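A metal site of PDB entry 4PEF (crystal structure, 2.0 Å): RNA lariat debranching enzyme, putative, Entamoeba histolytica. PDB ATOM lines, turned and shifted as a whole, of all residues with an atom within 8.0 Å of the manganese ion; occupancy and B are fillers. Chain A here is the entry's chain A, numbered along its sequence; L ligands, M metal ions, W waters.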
ATOM      1  N   CYS A  14     -11.096  -8.622 -26.746  1.00  0.00           N
ATOM      2  CA  CYS A  14     -10.454  -8.176 -27.984  1.00  0.00           C
ATOM      3  C   CYS A  14     -10.876  -6.778 -28.440  1.00  0.00           C
ATOM      4  O   CYS A  14     -12.044  -6.565 -28.799  1.00  0.00           O
ATOM      5  CB  CYS A  14     -10.785  -9.149 -29.112  1.00  0.00           C
ATOM      6  SG  CYS A  14     -10.229 -10.812 -28.781  1.00  0.00           S
ATOM      7  N   HIS A  16      -9.328  -5.059 -31.054  1.00  0.00           N
ATOM      8  CA  HIS A  16      -9.109  -5.009 -32.507  1.00  0.00           C
ATOM      9  C   HIS A  16      -9.223  -3.615 -33.131  1.00  0.00           C
ATOM     10  O   HIS A  16      -9.927  -3.411 -34.119  1.00  0.00           O
ATOM     11  CB  HIS A  16      -9.980  -6.039 -33.250  1.00  0.00           C
ATOM     12  CG  HIS A  16     -11.449  -5.808 -33.102  1.00  0.00           C
ATOM     13  ND1 HIS A  16     -12.135  -6.028 -31.929  1.00  0.00           N
ATOM     14  CD2 HIS A  16     -12.374  -5.365 -33.996  1.00  0.00           C
ATOM     15  CE1 HIS A  16     -13.408  -5.728 -32.098  1.00  0.00           C
ATOM     16  NE2 HIS A  16     -13.579  -5.327 -33.345  1.00  0.00           N
ATOM     17  N   THR A  43      -7.383  -7.653 -22.824  1.00  0.00           N
ATOM     18  CA  THR A  43      -6.710  -8.936 -22.962  1.00  0.00           C
ATOM     19  C   THR A  43      -6.099  -9.182 -24.353  1.00  0.00           C
ATOM     20  O   THR A  43      -5.767 -10.313 -24.694  1.00  0.00           O
ATOM     21  CB  THR A  43      -7.641 -10.113 -22.590  1.00  0.00           C
ATOM     22  OG1 THR A  43      -8.886  -9.944 -23.261  1.00  0.00           O
ATOM     23  CG2 THR A  43      -7.898 -10.160 -21.081  1.00  0.00           C
ATOM     24  N   GLY A  44      -5.965  -8.130 -25.167  1.00  0.00           N
ATOM     25  CA  GLY A  44      -5.203  -8.311 -26.396  1.00  0.00           C
ATOM     26  C   GLY A  44      -5.917  -8.091 -27.714  1.00  0.00           C
ATOM     27  O   GLY A  44      -7.082  -7.688 -27.749  1.00  0.00           O
ATOM     28  N   ASP A  45      -5.199  -8.385 -28.807  1.00  0.00           N
ATOM     29  CA  ASP A  45      -5.596  -7.947 -30.157  1.00  0.00           C
ATOM     30  C   ASP A  45      -5.778  -6.431 -30.184  1.00  0.00           C
ATOM     31  O   ASP A  45      -6.818  -5.922 -30.595  1.00  0.00           O
ATOM     32  CB  ASP A  45      -6.827  -8.707 -30.666  1.00  0.00           C
ATOM     33  CG  ASP A  45      -6.528 -10.163 -30.957  1.00  0.00           C
ATOM     34  OD1 ASP A  45      -5.316 -10.510 -30.995  1.00  0.00           O
ATOM     35  OD2 ASP A  45      -7.485 -10.952 -31.144  1.00  0.00           O
ATOM     36  N   MET A  46      -4.752  -5.728 -29.735  1.00  0.00           N
ATOM     37  CA  MET A  46      -4.831  -4.282 -29.606  1.00  0.00           C
ATOM     38  C   MET A  46      -4.588  -3.536 -30.900  1.00  0.00           C
ATOM     39  O   MET A  46      -5.114  -2.442 -31.082  1.00  0.00           O
ATOM     40  CB  MET A  46      -3.843  -3.799 -28.543  1.00  0.00           C
ATOM     41  CG  MET A  46      -3.954  -4.573 -27.261  1.00  0.00           C
ATOM     42  SD  MET A  46      -5.588  -4.401 -26.495  1.00  0.00           S
ATOM     43  CE  MET A  46      -5.631  -2.632 -26.189  1.00  0.00           C
ATOM     44  N   GLN A  47      -3.780  -4.103 -31.790  1.00  0.00           N
ATOM     45  CA  GLN A  47      -3.513  -3.499 -33.104  1.00  0.00           C
ATOM     46  C   GLN A  47      -3.025  -2.041 -32.973  1.00  0.00           C
ATOM     47  O   GLN A  47      -3.611  -1.100 -33.553  1.00  0.00           O
ATOM     48  CB  GLN A  47      -4.757  -3.596 -33.984  1.00  0.00           C
ATOM     49  CG  GLN A  47      -5.330  -5.015 -34.005  1.00  0.00           C
ATOM     50  CD  GLN A  47      -6.435  -5.250 -35.031  1.00  0.00           C
ATOM     51  OE1 GLN A  47      -6.706  -4.393 -35.880  1.00  0.00           O
ATOM     52  NE2 GLN A  47      -7.077  -6.406 -34.953  1.00  0.00           N
ATOM     53  N   GLY A  88      -0.437  -8.341 -25.432  1.00  0.00           N
ATOM     54  CA  GLY A  88      -0.651  -8.566 -26.843  1.00  0.00           C
ATOM     55  C   GLY A  88      -1.384  -9.871 -27.083  1.00  0.00           C
ATOM     56  O   GLY A  88      -1.338 -10.817 -26.276  1.00  0.00           O
ATOM     57  N   GLY A  89      -2.074  -9.933 -28.216  1.00  0.00           N
ATOM     58  CA  GLY A  89      -2.718 -11.164 -28.628  1.00  0.00           C
ATOM     59  C   GLY A  89      -2.084 -11.678 -29.913  1.00  0.00           C
ATOM     60  O   GLY A  89      -0.857 -11.687 -30.047  1.00  0.00           O
ATOM     61  N   ASN A  90      -2.927 -12.103 -30.850  1.00  0.00           N
ATOM     62  CA  ASN A  90      -2.439 -12.632 -32.122  1.00  0.00           C
ATOM     63  C   ASN A  90      -2.629 -11.662 -33.286  1.00  0.00           C
ATOM     64  O   ASN A  90      -2.122 -11.891 -34.384  1.00  0.00           O
ATOM     65  CB  ASN A  90      -3.096 -13.990 -32.457  1.00  0.00           C
ATOM     66  CG  ASN A  90      -4.609 -13.898 -32.530  1.00  0.00           C
ATOM     67  OD1 ASN A  90      -5.281 -13.654 -31.515  1.00  0.00           O
ATOM     68  ND2 ASN A  90      -5.170 -14.124 -33.713  1.00  0.00           N
ATOM     69  N   HIS A  91      -3.347 -10.568 -33.043  1.00  0.00           N
ATOM     70  CA  HIS A  91      -3.517  -9.496 -34.036  1.00  0.00           C
ATOM     71  C   HIS A  91      -2.910  -8.181 -33.524  1.00  0.00           C
ATOM     72  O   HIS A  91      -3.577  -7.401 -32.852  1.00  0.00           O
ATOM     73  CB  HIS A  91      -5.006  -9.266 -34.355  1.00  0.00           C
ATOM     74  CG  HIS A  91      -5.689 -10.435 -34.961  1.00  0.00           C
ATOM     75  ND1 HIS A  91      -5.181 -11.118 -36.045  1.00  0.00           N
ATOM     76  CD2 HIS A  91      -6.860 -11.054 -34.654  1.00  0.00           C
ATOM     77  CE1 HIS A  91      -6.001 -12.099 -36.372  1.00  0.00           C
ATOM     78  NE2 HIS A  91      -7.031 -12.081 -35.538  1.00  0.00           N
ATOM     79  N   GLU A  92      -1.645  -7.937 -33.854  1.00  0.00           N
ATOM     80  CA  GLU A  92      -0.916  -6.834 -33.229  1.00  0.00           C
ATOM     81  C   GLU A  92       0.027  -6.192 -34.211  1.00  0.00           C
ATOM     82  O   GLU A  92       0.430  -6.820 -35.186  1.00  0.00           O
ATOM     83  CB  GLU A  92      -0.074  -7.373 -32.054  1.00  0.00           C
ATOM     84  CG  GLU A  92      -0.856  -8.050 -30.943  1.00  0.00           C
ATOM     85  CD  GLU A  92      -1.776  -7.098 -30.181  1.00  0.00           C
ATOM     86  OE1 GLU A  92      -1.730  -5.855 -30.404  1.00  0.00           O
ATOM     87  OE2 GLU A  92      -2.555  -7.590 -29.341  1.00  0.00           O
ATOM     88  N   GLY A 131       0.453 -13.056 -26.244  1.00  0.00           N
ATOM     89  CA  GLY A 131       0.553 -13.999 -27.336  1.00  0.00           C
ATOM     90  C   GLY A 131      -0.422 -15.164 -27.331  1.00  0.00           C
ATOM     91  O   GLY A 131      -1.193 -15.347 -26.387  1.00  0.00           O
ATOM     92  N   ILE A 132      -0.395 -15.961 -28.411  1.00  0.00           N
ATOM     93  CA  ILE A 132      -1.085 -17.244 -28.431  1.00  0.00           C
ATOM     94  C   ILE A 132      -0.078 -18.400 -28.616  1.00  0.00           C
ATOM     95  O   ILE A 132       1.050 -18.202 -29.071  1.00  0.00           O
ATOM     96  CB  ILE A 132      -2.202 -17.305 -29.480  1.00  0.00           C
ATOM     97  CG1 ILE A 132      -1.638 -17.177 -30.897  1.00  0.00           C
ATOM     98  CG2 ILE A 132      -3.259 -16.224 -29.195  1.00  0.00           C
ATOM     99  CD1 ILE A 132      -2.650 -17.584 -31.976  1.00  0.00           C
ATOM    100  N   HIS A 180      -4.047 -13.959 -23.511  1.00  0.00           N
ATOM    101  CA  HIS A 180      -4.902 -13.825 -24.673  1.00  0.00           C
ATOM    102  C   HIS A 180      -5.663 -15.127 -24.915  1.00  0.00           C
ATOM    103  O   HIS A 180      -6.890 -15.165 -24.763  1.00  0.00           O
ATOM    104  CB  HIS A 180      -4.157 -13.365 -25.938  1.00  0.00           C
ATOM    105  CG  HIS A 180      -5.094 -12.973 -27.030  1.00  0.00           C
ATOM    106  ND1 HIS A 180      -5.944 -11.898 -26.926  1.00  0.00           N
ATOM    107  CD2 HIS A 180      -5.370 -13.572 -28.218  1.00  0.00           C
ATOM    108  CE1 HIS A 180      -6.674 -11.818 -28.022  1.00  0.00           C
ATOM    109  NE2 HIS A 180      -6.361 -12.828 -28.816  1.00  0.00           N
ATOM    110  N   ASP A 181      -4.958 -16.202 -25.273  1.00  0.00           N
ATOM    111  CA  ASP A 181      -5.691 -17.458 -25.362  1.00  0.00           C
ATOM    112  C   ASP A 181      -5.930 -18.027 -23.955  1.00  0.00           C
ATOM    113  O   ASP A 181      -5.293 -17.583 -22.983  1.00  0.00           O
ATOM    114  CB  ASP A 181      -5.083 -18.467 -26.359  1.00  0.00           C
ATOM    115  CG  ASP A 181      -3.604 -18.715 -26.160  1.00  0.00           C
ATOM    116  OD1 ASP A 181      -2.949 -18.028 -25.328  1.00  0.00           O
ATOM    117  OD2 ASP A 181      -3.085 -19.599 -26.875  1.00  0.00           O
ATOM    118  N   GLY A 229      -9.006 -13.305 -23.424  1.00  0.00           N
ATOM    119  CA  GLY A 229      -9.817 -12.895 -24.554  1.00  0.00           C
ATOM    120  C   GLY A 229      -9.801 -13.974 -25.624  1.00  0.00           C
ATOM    121  O   GLY A 229      -9.993 -15.168 -25.336  1.00  0.00           O
ATOM    122  N   HIS A 230      -9.569 -13.553 -26.862  1.00  0.00           N
ATOM    123  CA  HIS A 230      -9.366 -14.488 -27.992  1.00  0.00           C
ATOM    124  C   HIS A 230     -10.586 -15.267 -28.491  1.00  0.00           C
ATOM    125  O   HIS A 230     -10.766 -15.388 -29.702  1.00  0.00           O
ATOM    126  CB  HIS A 230      -8.199 -15.469 -27.729  1.00  0.00           C
ATOM    127  CG  HIS A 230      -7.728 -16.168 -28.980  1.00  0.00           C
ATOM    128  ND1 HIS A 230      -7.488 -15.504 -30.150  1.00  0.00           N
ATOM    129  CD2 HIS A 230      -7.461 -17.474 -29.216  1.00  0.00           C
ATOM    130  CE1 HIS A 230      -7.091 -16.368 -31.074  1.00  0.00           C
ATOM    131  NE2 HIS A 230      -7.060 -17.560 -30.527  1.00  0.00           N
ATOM    132  N   MET A 231     -11.402 -15.803 -27.594  1.00  0.00           N
ATOM    133  CA  MET A 231     -12.430 -16.770 -28.019  1.00  0.00           C
ATOM    134  C   MET A 231     -13.788 -16.193 -28.443  1.00  0.00           C
ATOM    135  O   MET A 231     -14.670 -16.937 -28.882  1.00  0.00           O
ATOM    136  CB  MET A 231     -12.642 -17.895 -26.985  1.00  0.00           C
ATOM    137  CG  MET A 231     -11.461 -18.851 -26.777  1.00  0.00           C
ATOM    138  SD  MET A 231     -10.740 -19.573 -28.265  1.00  0.00           S
ATOM    139  CE  MET A 231     -12.093 -20.576 -28.855  1.00  0.00           C
ATOM    140  N   HIS A 232     -13.972 -14.883 -28.300  1.00  0.00           N
ATOM    141  CA  HIS A 232     -15.200 -14.204 -28.751  1.00  0.00           C
ATOM    142  C   HIS A 232     -16.478 -14.624 -28.033  1.00  0.00           C
ATOM    143  O   HIS A 232     -17.538 -14.639 -28.625  1.00  0.00           O
ATOM    144  CB  HIS A 232     -15.419 -14.393 -30.246  1.00  0.00           C
ATOM    145  CG  HIS A 232     -14.376 -13.759 -31.107  1.00  0.00           C
ATOM    146  ND1 HIS A 232     -14.441 -13.771 -32.485  1.00  0.00           N
ATOM    147  CD2 HIS A 232     -13.241 -13.085 -30.782  1.00  0.00           C
ATOM    148  CE1 HIS A 232     -13.393 -13.128 -32.972  1.00  0.00           C
ATOM    149  NE2 HIS A 232     -12.654 -12.705 -31.967  1.00  0.00           N
HETATM  150  S1  LIG L   1      -9.318 -13.951 -33.587  1.00  0.00           S
HETATM  151  O1  LIG L   1      -9.190 -13.664 -35.014  1.00  0.00           O
HETATM  152  O2  LIG L   1      -7.987 -13.986 -32.984  1.00  0.00           O
HETATM  153  O3  LIG L   1      -9.986 -15.251 -33.380  1.00  0.00           O
HETATM  154  O4  LIG L   1     -10.125 -12.901 -32.970  1.00  0.00           O
HETATM  155 MN    MN M   1      -7.285 -13.146 -30.899  1.00  0.00          MN
HETATM  156  O   HOH W   1      -9.337 -12.531 -30.437  1.00  0.00           O
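Water W1 bridges the side-chain sulfur (SG) of Cys 14 (2.5 Å) and the backbone carbonyl oxygen (O) of His 230 (3.3 Å).
Within 4 Å of the manganese ion: Asp 45, Asn 90, His 180 and His 230.
The manganese ion is bound by OD1 of Asn 90, water W1, OD2 of Asp 45, NE2 of His 180, O2 of the ligand and ND1 of His 230.
ND2 of Asn 90 lies within hydrogen-bond range of NE2 of His 91 (3.3 Å).
The side-chain sulfur (SG) of Cys 14 lies close to the side-chain carboxylate (OD2) of Asp 45 (3.6 Å).
The side-chain carboxylate (OD1) of Asp 45 is in hydrogen-bond range of the backbone NH (N) of His 91, at 2.8 Å.
The side-chain carboxylate of Glu 92 lies within hydrogen-bond range of the backbone NH of Asp 45, at 2.8 Å.
N of His 16 sits at hydrogen-bond distance from O of Asp 45, 2.7 Å away.
N of Gly 229 sits at hydrogen-bond distance from O of His 180.
A ring nitrogen (ND1) of His 180 is in hydrogen-bond range of the backbone carbonyl oxygen of Thr 43 (2.7 Å).
The side-chain sulfur of Cys 14 lies within hydrogen-bond range of the backbone NH of His 230 (3.4 Å).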
